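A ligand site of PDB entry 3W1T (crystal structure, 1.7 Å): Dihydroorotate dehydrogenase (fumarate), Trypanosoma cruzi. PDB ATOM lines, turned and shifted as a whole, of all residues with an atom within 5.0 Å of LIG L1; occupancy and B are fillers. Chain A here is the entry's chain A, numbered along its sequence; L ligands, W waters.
OD1 of Asn 195 lies within hydrogen-bond range of N2 of LG2 L2. The backbone NH (N) of Leu 72 is in hydrogen-bond range of an oxygen (O1) of LG2 L2 (2.9 Å). An oxygen (O8) of LIG L1 sits at hydrogen-bond distance from the backbone NH of Gly 223 (2.8 Å). The backbone NH of Gly 272 is in hydrogen-bond range of an oxygen (O7) of LIG L1 (3.0 Å). N of Met 70 is in hydrogen-bond range of O2 of LG2 L2, 3.1 Å away. The backbone NH (N) of Thr 273 is in hydrogen-bond range of an oxygen (O9) of LIG L1 (2.8 Å). O3 of LIG L1 is in hydrogen-bond range of O of Ala 20, at 2.8 Å. The side-chain amide oxygen of Asn 68 lies within hydrogen-bond range of a nitrogen (N1) of LG2 L2, 2.9 Å away. The side-chain amino group (NZ) of Lys 44 sits at hydrogen-bond distance from an oxygen (O2) of LIG L1, 2.7 Å away. O3 of LG2 L2 is in hydrogen-bond range of OG of Ser 196 (3.0 Å). The side-chain amide nitrogen (ND2) of Asn 128 lies within hydrogen-bond range of an oxygen (O4) of LG2 L2, 3.0 Å away. O of Val 194 lies within hydrogen-bond range of O4 of LIG L1. O3 of LIG L1 is in hydrogen-bond range of NZ of Lys 165 (2.9 Å). NZ of Lys 44 lies within salt-bridge range of O1 of LG2 L2, 3.2 Å away. O1 of LIG L1 sits at hydrogen-bond distance from ND2 of Asn 195 (3.4 Å). The side-chain hydroxyl of Thr 273 lies within hydrogen-bond range of an oxygen (O9) of LIG L1 (2.7 Å). A nitrogen (N2) of LIG L1 is in hydrogen-bond range of the side-chain hydroxyl (OG) of Ser 45, 2.7 Å away. N of Gly 251 lies within hydrogen-bond range of O8 of LIG L1 (2.8 Å). An oxygen (O4) of LIG L1 sits at hydrogen-bond distance from the side-chain sulfur (SG) of Cys 249 (3.5 Å). The side-chain amide nitrogen (ND2) of Asn 128 lies within hydrogen-bond range of an oxygen (O1) of LIG L1 (3.4 Å).
A nitrogen (N1) of LIG L1 lies close to a nitrogen (N2) of LG2 L2, 3.4 Å away.
The side-chain amide oxygen (OE1) of Gln 270 lies within hydrogen-bond range of the side-chain sulfur (SG) of Cys 249. The side-chain hydroxyl (OG) of Ser 45 sits at hydrogen-bond distance from the side-chain hydroxyl (OG) of Ser 98 (2.6 Å). The backbone NH (N) of Val 194 is in hydrogen-bond range of the backbone carbonyl oxygen (O) of Cys 249, at 2.9 Å. The backbone carbonyl oxygen of Gly 222 lies within hydrogen-bond range of the backbone NH of Ser 66 (2.9 Å). The backbone carbonyl oxygen (O) of Val 271 lies within hydrogen-bond range of the backbone NH (N) of Ala 19 (2.9 Å). The side-chain hydroxyl of Thr 273 sits at hydrogen-bond distance from the side-chain hydroxyl of Ser 66, 2.7 Å away. ND2 of Asn 195 sits at hydrogen-bond distance from OD1 of Asn 128. N of Met 70 lies close to OD1 of Asn 68 (3.4 Å).
Ala 19 touches LIG L1. Gly 21 touches LIG L1. Tyr 59 touches LIG L1. ND2 of Asn 68 touches C8 of LIG L1, at 3.5 Å. Met 70 touches LIG L1. Ser 196 touches LIG L1 (N to O4, 3.98 Å). Gly 222 touches LIG L1 (CA to O8, 3.7 Å). CD1 of Ile 226 touches O8 of LIG L1, at 3.6 Å. Gly 250 touches LIG L1 (CA to O8, 3.3 Å). Hydrophobic or aromatic side chains within 4 Å of LIG L1: Ala 19, Ala 20, Tyr 59, Met 70 and Ile 226. 21 residues have an atom within 4 Å of LIG L1: Ala 19, Ala 20, Gly 21, Lys 44, Ser 45, Tyr 59, Asn 68, Met 70, Asn 128, Lys 165, Val 194, Asn 195, Ser 196, Gly 222, Gly 223, Ile 226, Cys 249, Gly 250, Gly 251, Gly 272 and Thr 273.
Water W3 lies within hydrogen-bond range of O7 of LIG L1 (2.7 Å), N of Ala 274 (2.8 Å) and O of Val 252 (2.9 Å). Water W2 lies within hydrogen-bond range of the side-chain hydroxyl of Ser 98 (2.6 Å), the side-chain carboxylate of Glu 126 (2.7 Å) and an oxygen (O1) of LIG L1 (2.8 Å).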
ATOM      1  N   ALA A  19      11.547   3.290   2.682  1.00  0.00           N
ATOM      2  CA  ALA A  19      12.231   3.312   3.955  1.00  0.00           C
ATOM      3  C   ALA A  19      11.268   3.128   5.123  1.00  0.00           C
ATOM      4  O   ALA A  19      10.157   3.608   5.087  1.00  0.00           O
ATOM      5  CB  ALA A  19      12.910   4.660   4.073  1.00  0.00           C
ATOM      6  N   ALA A  20      11.683   2.379   6.154  1.00  0.00           N
ATOM      7  CA  ALA A  20      10.773   2.135   7.263  1.00  0.00           C
ATOM      8  C   ALA A  20      10.280   3.490   7.799  1.00  0.00           C
ATOM      9  O   ALA A  20      11.042   4.466   7.865  1.00  0.00           O
ATOM     10  CB  ALA A  20      11.414   1.328   8.379  1.00  0.00           C
ATOM     11  N   GLY A  21       8.991   3.505   8.127  1.00  0.00           N
ATOM     12  CA  GLY A  21       8.321   4.678   8.592  1.00  0.00           C
ATOM     13  C   GLY A  21       7.578   5.492   7.566  1.00  0.00           C
ATOM     14  O   GLY A  21       6.702   6.205   7.913  1.00  0.00           O
ATOM     15  N   VAL A  22       7.874   5.260   6.310  1.00  0.00           N
ATOM     16  CA  VAL A  22       7.193   6.014   5.270  1.00  0.00           C
ATOM     17  C   VAL A  22       6.201   5.134   4.496  1.00  0.00           C
ATOM     18  O   VAL A  22       6.562   4.175   4.025  1.00  0.00           O
ATOM     19  CB  VAL A  22       8.218   6.637   4.312  1.00  0.00           C
ATOM     20  CG1 VAL A  22       7.560   7.347   3.148  1.00  0.00           C
ATOM     21  CG2 VAL A  22       9.072   7.588   5.104  1.00  0.00           C
ATOM     22  N   LYS A  44       6.268  -0.284   9.099  1.00  0.00           N
ATOM     23  CA  LYS A  44       6.651   0.640  10.134  1.00  0.00           C
ATOM     24  C   LYS A  44       7.269  -0.090  11.329  1.00  0.00           C
ATOM     25  O   LYS A  44       6.673  -1.038  11.837  1.00  0.00           O
ATOM     26  CB  LYS A  44       5.429   1.392  10.616  1.00  0.00           C
ATOM     27  CG  LYS A  44       5.643   2.356  11.767  1.00  0.00           C
ATOM     28  CD  LYS A  44       6.528   3.534  11.492  1.00  0.00           C
ATOM     29  CE  LYS A  44       6.992   4.315  12.768  1.00  0.00           C
ATOM     30  NZ  LYS A  44       7.955   5.569  12.724  1.00  0.00           N
ATOM     31  N   SER A  45       8.405   0.442  11.823  1.00  0.00           N
ATOM     32  CA  SER A  45       9.064  -0.077  13.033  1.00  0.00           C
ATOM     33  C   SER A  45       8.012  -0.144  14.087  1.00  0.00           C
ATOM     34  O   SER A  45       7.294   0.824  14.320  1.00  0.00           O
ATOM     35  CB  SER A  45      10.203   0.817  13.522  1.00  0.00           C
ATOM     36  OG  SER A  45      11.251   0.702  12.566  1.00  0.00           O
ATOM     37  N   TYR A  59       6.555  16.031  11.743  1.00  0.00           N
ATOM     38  CA  TYR A  59       7.275  15.884  10.461  1.00  0.00           C
ATOM     39  C   TYR A  59       7.081  17.126   9.634  1.00  0.00           C
ATOM     40  O   TYR A  59       5.968  17.623   9.496  1.00  0.00           O
ATOM     41  CB  TYR A  59       6.746  14.711   9.663  1.00  0.00           C
ATOM     42  CG  TYR A  59       7.263  14.575   8.247  1.00  0.00           C
ATOM     43  CD1 TYR A  59       8.486  13.957   7.952  1.00  0.00           C
ATOM     44  CD2 TYR A  59       6.583  15.155   7.193  1.00  0.00           C
ATOM     45  CE1 TYR A  59       8.978  13.888   6.661  1.00  0.00           C
ATOM     46  CE2 TYR A  59       7.052  15.082   5.897  1.00  0.00           C
ATOM     47  CZ  TYR A  59       8.228  14.453   5.594  1.00  0.00           C
ATOM     48  OH  TYR A  59       8.713  14.340   4.281  1.00  0.00           O
ATOM     49  N   SER A  66      13.890  16.662   5.038  1.00  0.00           N
ATOM     50  CA  SER A  66      12.862  16.580   6.021  1.00  0.00           C
ATOM     51  C   SER A  66      13.516  16.481   7.412  1.00  0.00           C
ATOM     52  O   SER A  66      14.673  16.160   7.568  1.00  0.00           O
ATOM     53  CB  SER A  66      11.944  15.381   5.776  1.00  0.00           C
ATOM     54  OG  SER A  66      12.676  14.166   6.017  1.00  0.00           O
ATOM     55  N   ASN A  68      12.130  15.048  11.399  1.00  0.00           N
ATOM     56  CA  ASN A  68      11.052  14.408  12.135  1.00  0.00           C
ATOM     57  C   ASN A  68      11.430  13.968  13.536  1.00  0.00           C
ATOM     58  O   ASN A  68      12.547  13.570  13.791  1.00  0.00           O
ATOM     59  CB  ASN A  68      10.531  13.180  11.352  1.00  0.00           C
ATOM     60  CG  ASN A  68      11.310  11.919  11.669  1.00  0.00           C
ATOM     61  OD1 ASN A  68      11.057  11.217  12.655  1.00  0.00           O
ATOM     62  ND2 ASN A  68      12.201  11.573  10.802  1.00  0.00           N
ATOM     63  N   MET A  70       8.934  11.735  15.231  1.00  0.00           N
ATOM     64  CA  MET A  70       7.603  11.141  15.253  1.00  0.00           C
ATOM     65  C   MET A  70       7.243  10.443  16.566  1.00  0.00           C
ATOM     66  O   MET A  70       6.073  10.384  16.933  1.00  0.00           O
ATOM     67  CB  MET A  70       7.510  10.110  14.195  1.00  0.00           C
ATOM     68  CG  MET A  70       7.802  10.460  12.765  1.00  0.00           C
ATOM     69  SD  MET A  70       6.746  11.675  12.066  1.00  0.00           S
ATOM     70  CE  MET A  70       5.244  10.802  11.822  1.00  0.00           C
ATOM     71  N   LEU A  72       7.784   7.202  17.253  1.00  0.00           N
ATOM     72  CA  LEU A  72       7.455   5.813  16.958  1.00  0.00           C
ATOM     73  C   LEU A  72       5.957   5.515  17.055  1.00  0.00           C
ATOM     74  O   LEU A  72       5.559   4.477  17.630  1.00  0.00           O
ATOM     75  CB  LEU A  72       8.316   4.860  17.788  1.00  0.00           C
ATOM     76  CG  LEU A  72       8.501   3.378  17.435  1.00  0.00           C
ATOM     77  CD1 LEU A  72       8.895   3.213  15.985  1.00  0.00           C
ATOM     78  CD2 LEU A  72       9.639   2.931  18.400  1.00  0.00           C
ATOM     79  N   SER A  98       9.852  -4.393  10.161  1.00  0.00           N
ATOM     80  CA  SER A  98      10.811  -3.704  11.015  1.00  0.00           C
ATOM     81  C   SER A  98      10.341  -3.666  12.453  1.00  0.00           C
ATOM     82  O   SER A  98       9.136  -3.423  12.723  1.00  0.00           O
ATOM     83  CB  SER A  98      11.008  -2.277  10.546  1.00  0.00           C
ATOM     84  OG  SER A  98      11.851  -1.532  11.487  1.00  0.00           O
ATOM     85  N   GLU A 126      13.887  -6.631   9.721  1.00  0.00           N
ATOM     86  CA  GLU A 126      14.822  -5.489   9.825  1.00  0.00           C
ATOM     87  C   GLU A 126      14.730  -4.960  11.255  1.00  0.00           C
ATOM     88  O   GLU A 126      13.718  -4.416  11.694  1.00  0.00           O
ATOM     89  CB  GLU A 126      14.557  -4.364   8.802  1.00  0.00           C
ATOM     90  CG  GLU A 126      15.586  -3.283   8.790  1.00  0.00           C
ATOM     91  CD  GLU A 126      15.323  -2.232   7.712  1.00  0.00           C
ATOM     92  OE1 GLU A 126      14.517  -1.296   7.993  1.00  0.00           O
ATOM     93  OE2 GLU A 126      15.907  -2.325   6.575  1.00  0.00           O
ATOM     94  N   ASN A 128      15.678  -2.352  13.962  1.00  0.00           N
ATOM     95  CA  ASN A 128      16.084  -0.989  14.007  1.00  0.00           C
ATOM     96  C   ASN A 128      16.884  -0.713  15.296  1.00  0.00           C
ATOM     97  O   ASN A 128      16.345  -0.670  16.358  1.00  0.00           O
ATOM     98  CB  ASN A 128      14.866  -0.096  13.995  1.00  0.00           C
ATOM     99  CG  ASN A 128      15.199   1.372  14.059  1.00  0.00           C
ATOM    100  OD1 ASN A 128      16.263   1.758  13.980  1.00  0.00           O
ATOM    101  ND2 ASN A 128      14.211   2.147  14.183  1.00  0.00           N
ATOM    102  N   LYS A 165      19.006  -2.023  10.759  1.00  0.00           N
ATOM    103  CA  LYS A 165      18.944  -0.623  10.321  1.00  0.00           C
ATOM    104  C   LYS A 165      19.865   0.238  11.204  1.00  0.00           C
ATOM    105  O   LYS A 165      19.744   0.195  12.432  1.00  0.00           O
ATOM    106  CB  LYS A 165      17.522  -0.133  10.374  1.00  0.00           C
ATOM    107  CG  LYS A 165      17.355   1.312   9.950  1.00  0.00           C
ATOM    108  CD  LYS A 165      17.422   1.545   8.470  1.00  0.00           C
ATOM    109  CE  LYS A 165      16.899   2.923   8.100  1.00  0.00           C
ATOM    110  NZ  LYS A 165      15.437   3.047   8.199  1.00  0.00           N
ATOM    111  N   VAL A 194      21.287   4.431   5.635  1.00  0.00           N
ATOM    112  CA  VAL A 194      21.262   4.843   7.029  1.00  0.00           C
ATOM    113  C   VAL A 194      19.895   5.278   7.448  1.00  0.00           C
ATOM    114  O   VAL A 194      19.049   5.653   6.641  1.00  0.00           O
ATOM    115  CB  VAL A 194      22.221   6.069   7.295  1.00  0.00           C
ATOM    116  CG1 VAL A 194      23.625   5.662   7.012  1.00  0.00           C
ATOM    117  CG2 VAL A 194      21.856   7.242   6.372  1.00  0.00           C
ATOM    118  N   ASN A 195      19.725   5.298   8.771  1.00  0.00           N
ATOM    119  CA  ASN A 195      18.611   6.017   9.396  1.00  0.00           C
ATOM    120  C   ASN A 195      18.899   7.541   9.339  1.00  0.00           C
ATOM    121  O   ASN A 195      19.861   7.950   8.836  1.00  0.00           O
ATOM    122  CB  ASN A 195      18.429   5.539  10.863  1.00  0.00           C
ATOM    123  CG  ASN A 195      16.990   5.550  11.321  1.00  0.00           C
ATOM    124  OD1 ASN A 195      16.363   6.480  11.141  1.00  0.00           O
ATOM    125  ND2 ASN A 195      16.541   4.482  11.927  1.00  0.00           N
ATOM    126  N   SER A 196      17.987   8.331   9.885  1.00  0.00           N
ATOM    127  CA  SER A 196      18.100   9.759   9.718  1.00  0.00           C
ATOM    128  C   SER A 196      19.326  10.286  10.440  1.00  0.00           C
ATOM    129  O   SER A 196      19.821   9.665  11.321  1.00  0.00           O
ATOM    130  CB  SER A 196      16.825  10.441  10.223  1.00  0.00           C
ATOM    131  OG  SER A 196      16.482  10.038  11.434  1.00  0.00           O
ATOM    132  N   GLY A 222      16.368  13.771   6.970  1.00  0.00           N
ATOM    133  CA  GLY A 222      16.437  13.023   5.762  1.00  0.00           C
ATOM    134  C   GLY A 222      16.511  13.906   4.540  1.00  0.00           C
ATOM    135  O   GLY A 222      16.318  15.139   4.579  1.00  0.00           O
ATOM    136  N   GLY A 223      16.653  13.243   3.433  1.00  0.00           N
ATOM    137  CA  GLY A 223      16.557  13.871   2.170  1.00  0.00           C
ATOM    138  C   GLY A 223      17.899  14.353   1.593  1.00  0.00           C
ATOM    139  O   GLY A 223      18.950  13.754   1.801  1.00  0.00           O
ATOM    140  N   ILE A 226      21.345  14.547   3.335  1.00  0.00           N
ATOM    141  CA  ILE A 226      22.044  13.424   3.881  1.00  0.00           C
ATOM    142  C   ILE A 226      22.681  12.470   2.848  1.00  0.00           C
ATOM    143  O   ILE A 226      23.268  11.493   3.206  1.00  0.00           O
ATOM    144  CB  ILE A 226      21.234  12.650   4.888  1.00  0.00           C
ATOM    145  CG1 ILE A 226      20.182  11.736   4.272  1.00  0.00           C
ATOM    146  CG2 ILE A 226      20.609  13.568   5.945  1.00  0.00           C
ATOM    147  CD1 ILE A 226      19.661  10.687   5.210  1.00  0.00           C
ATOM    148  N   CYS A 249      19.971   3.558   2.055  1.00  0.00           N
ATOM    149  CA  CYS A 249      18.880   4.497   2.409  1.00  0.00           C
ATOM    150  C   CYS A 249      19.426   5.852   2.719  1.00  0.00           C
ATOM    151  O   CYS A 249      20.400   6.043   3.454  1.00  0.00           O
ATOM    152  CB  CYS A 249      18.102   3.983   3.563  1.00  0.00           C
ATOM    153  SG  CYS A 249      16.576   4.849   3.942  1.00  0.00           S
ATOM    154  N   GLY A 250      18.868   6.871   2.059  1.00  0.00           N
ATOM    155  CA  GLY A 250      19.162   8.245   2.373  1.00  0.00           C
ATOM    156  C   GLY A 250      19.405   9.129   1.136  1.00  0.00           C
ATOM    157  O   GLY A 250      20.314   8.911   0.323  1.00  0.00           O
ATOM    158  N   GLY A 251      18.599  10.176   1.032  1.00  0.00           N
ATOM    159  CA  GLY A 251      18.749  11.120  -0.064  1.00  0.00           C
ATOM    160  C   GLY A 251      18.385  10.638  -1.453  1.00  0.00           C
ATOM    161  O   GLY A 251      18.868  11.248  -2.401  1.00  0.00           O
ATOM    162  N   VAL A 252      17.656   9.531  -1.584  1.00  0.00           N
ATOM    163  CA  VAL A 252      17.293   9.080  -2.968  1.00  0.00           C
ATOM    164  C   VAL A 252      16.092   9.862  -3.448  1.00  0.00           C
ATOM    165  O   VAL A 252      14.995   9.671  -2.906  1.00  0.00           O
ATOM    166  CB  VAL A 252      17.050   7.553  -3.058  1.00  0.00           C
ATOM    167  CG1 VAL A 252      16.568   7.089  -4.442  1.00  0.00           C
ATOM    168  CG2 VAL A 252      18.343   6.829  -2.636  1.00  0.00           C
ATOM    169  N   GLN A 270      16.362   2.074  -0.538  1.00  0.00           N
ATOM    170  CA  GLN A 270      15.148   2.474   0.150  1.00  0.00           C
ATOM    171  C   GLN A 270      14.974   4.007  -0.084  1.00  0.00           C
ATOM    172  O   GLN A 270      15.946   4.757  -0.160  1.00  0.00           O
ATOM    173  CB  GLN A 270      15.227   2.223   1.661  1.00  0.00           C
ATOM    174  CG  GLN A 270      15.681   0.809   1.969  1.00  0.00           C
ATOM    175  CD  GLN A 270      15.548   0.458   3.436  1.00  0.00           C
ATOM    176  OE1 GLN A 270      15.623   1.332   4.313  1.00  0.00           O
ATOM    177  NE2 GLN A 270      15.443  -0.822   3.734  1.00  0.00           N
ATOM    178  N   VAL A 271      13.703   4.431  -0.041  1.00  0.00           N
ATOM    179  CA  VAL A 271      13.288   5.748  -0.347  1.00  0.00           C
ATOM    180  C   VAL A 271      12.321   6.205   0.755  1.00  0.00           C
ATOM    181  O   VAL A 271      11.207   5.627   0.922  1.00  0.00           O
ATOM    182  CB  VAL A 271      12.566   5.794  -1.700  1.00  0.00           C
ATOM    183  CG1 VAL A 271      12.359   7.242  -2.116  1.00  0.00           C
ATOM    184  CG2 VAL A 271      13.354   5.035  -2.792  1.00  0.00           C
ATOM    185  N   GLY A 272      12.713   7.238   1.475  1.00  0.00           N
ATOM    186  CA  GLY A 272      11.969   7.805   2.623  1.00  0.00           C
ATOM    187  C   GLY A 272      11.356   9.137   2.194  1.00  0.00           C
ATOM    188  O   GLY A 272      10.262   9.164   1.653  1.00  0.00           O
ATOM    189  N   THR A 273      12.054  10.211   2.495  1.00  0.00           N
ATOM    190  CA  THR A 273      11.556  11.575   2.329  1.00  0.00           C
ATOM    191  C   THR A 273      10.970  11.780   0.905  1.00  0.00           C
ATOM    192  O   THR A 273       9.877  12.264   0.762  1.00  0.00           O
ATOM    193  CB  THR A 273      12.710  12.590   2.544  1.00  0.00           C
ATOM    194  OG1 THR A 273      13.171  12.529   3.924  1.00  0.00           O
ATOM    195  CG2 THR A 273      12.277  14.043   2.312  1.00  0.00           C
ATOM    196  N   ALA A 274      11.698  11.335  -0.141  1.00  0.00           N
ATOM    197  CA  ALA A 274      11.192  11.608  -1.502  1.00  0.00           C
ATOM    198  C   ALA A 274       9.869  10.907  -1.744  1.00  0.00           C
ATOM    199  O   ALA A 274       9.019  11.412  -2.449  1.00  0.00           O
ATOM    200  CB  ALA A 274      12.228  11.262  -2.511  1.00  0.00           C
HETATM  201  N1  LIG L   1      13.488   4.483  10.225  1.00  0.00           N
HETATM  202  C1  LIG L   1      13.209   3.318  10.832  1.00  0.00           C
HETATM  203  O1  LIG L   1      14.087   2.430  10.769  1.00  0.00           O
HETATM  204  N2  LIG L   1      12.017   3.080  11.479  1.00  0.00           N
HETATM  205  C2  LIG L   1      11.033   3.983  11.501  1.00  0.00           C
HETATM  206  O2  LIG L   1       9.902   3.809  12.044  1.00  0.00           O
HETATM  207  C3  LIG L   1      11.218   5.238  10.790  1.00  0.00           C
HETATM  208  N3  LIG L   1      10.256   6.191  10.818  1.00  0.00           N
HETATM  209  C4  LIG L   1      10.438   7.291  10.057  1.00  0.00           C
HETATM  210  C5  LIG L   1       9.360   8.211   9.896  1.00  0.00           C
HETATM  211  C6  LIG L   1       9.468   9.331   9.119  1.00  0.00           C
HETATM  212  C7  LIG L   1       8.327  10.302   8.967  1.00  0.00           C
HETATM  213  C8  LIG L   1      10.695   9.542   8.377  1.00  0.00           C
HETATM  214  C9  LIG L   1      10.852  10.769   7.550  1.00  0.00           C
HETATM  215  C10 LIG L   1      11.764   8.654   8.523  1.00  0.00           C
HETATM  216  C11 LIG L   1      11.646   7.471   9.269  1.00  0.00           C
HETATM  217  N4  LIG L   1      12.711   6.586   9.456  1.00  0.00           N
HETATM  218  C12 LIG L   1      12.519   5.425  10.162  1.00  0.00           C
HETATM  219  C13 LIG L   1      13.990   6.780   8.755  1.00  0.00           C
HETATM  220  C14 LIG L   1      13.852   6.450   7.298  1.00  0.00           C
HETATM  221  O3  LIG L   1      13.655   5.085   7.205  1.00  0.00           O
HETATM  222  C15 LIG L   1      15.139   6.772   6.630  1.00  0.00           C
HETATM  223  O4  LIG L   1      16.214   5.992   7.196  1.00  0.00           O
HETATM  224  C16 LIG L   1      15.537   8.275   6.646  1.00  0.00           C
HETATM  225  O5  LIG L   1      14.372   9.059   6.447  1.00  0.00           O
HETATM  226  C17 LIG L   1      16.515   8.602   5.503  1.00  0.00           C
HETATM  227  O6  LIG L   1      16.106   8.278   4.152  1.00  0.00           O
HETATM  228  P1  LIG L   1      15.599   9.517   3.259  1.00  0.00           P
HETATM  229  O7  LIG L   1      15.124   8.857   1.995  1.00  0.00           O
HETATM  230  O8  LIG L   1      16.751  10.451   3.067  1.00  0.00           O
HETATM  231  O9  LIG L   1      14.444  10.181   4.008  1.00  0.00           O
HETATM  232  O1  LG2 L   2       9.527   7.295  14.944  1.00  0.00           O
HETATM  233  C1  LG2 L   2      10.540   7.996  14.883  1.00  0.00           C
HETATM  234  O2  LG2 L   2      10.681   9.132  15.369  1.00  0.00           O
HETATM  235  C2  LG2 L   2      11.719   7.554  14.088  1.00  0.00           C
HETATM  236  N1  LG2 L   2      12.117   8.518  13.160  1.00  0.00           N
HETATM  237  C3  LG2 L   2      13.226   8.276  12.301  1.00  0.00           C
HETATM  238  O3  LG2 L   2      13.667   9.121  11.533  1.00  0.00           O
HETATM  239  N2  LG2 L   2      13.880   7.057  12.440  1.00  0.00           N
HETATM  240  C4  LG2 L   2      13.526   6.084  13.417  1.00  0.00           C
HETATM  241  O4  LG2 L   2      14.178   5.041  13.520  1.00  0.00           O
HETATM  242  C5  LG2 L   2      12.391   6.357  14.243  1.00  0.00           C
HETATM  243  C6  LG2 L   2      11.989   5.428  15.193  1.00  0.00           C
HETATM  244  C7  LG2 L   2      13.031   5.291  16.319  1.00  0.00           C
HETATM  245  C8  LG2 L   2      12.846   6.157  17.326  1.00  0.00           C
HETATM  246  C9  LG2 L   2      11.957   5.848  18.425  1.00  0.00           C
HETATM  247  C10 LG2 L   2      11.767   6.817  19.432  1.00  0.00           C
HETATM  248  C11 LG2 L   2      10.869   6.559  20.589  1.00  0.00           C
HETATM  249  F1  LG2 L   2      10.499   5.424  20.846  1.00  0.00           F
HETATM  250  F2  LG2 L   2      11.443   6.899  21.598  1.00  0.00           F
HETATM  251  F3  LG2 L   2       9.796   7.162  20.381  1.00  0.00           F
HETATM  252  C12 LG2 L   2      12.428   8.085  19.351  1.00  0.00           C
HETATM  253  C13 LG2 L   2      13.312   8.389  18.289  1.00  0.00           C
HETATM  254  C14 LG2 L   2      13.517   7.402  17.290  1.00  0.00           C
HETATM  255  O   HOH W   1      14.658  10.724   8.278  1.00  0.00           O
HETATM  256  O   HOH W   2      14.001  -0.401  10.454  1.00  0.00           O
HETATM  257  O   HOH W   3      14.363  10.364  -0.132  1.00  0.00           O
HETATM  258  O   HOH W   4      16.681   7.459   0.373  1.00  0.00           O
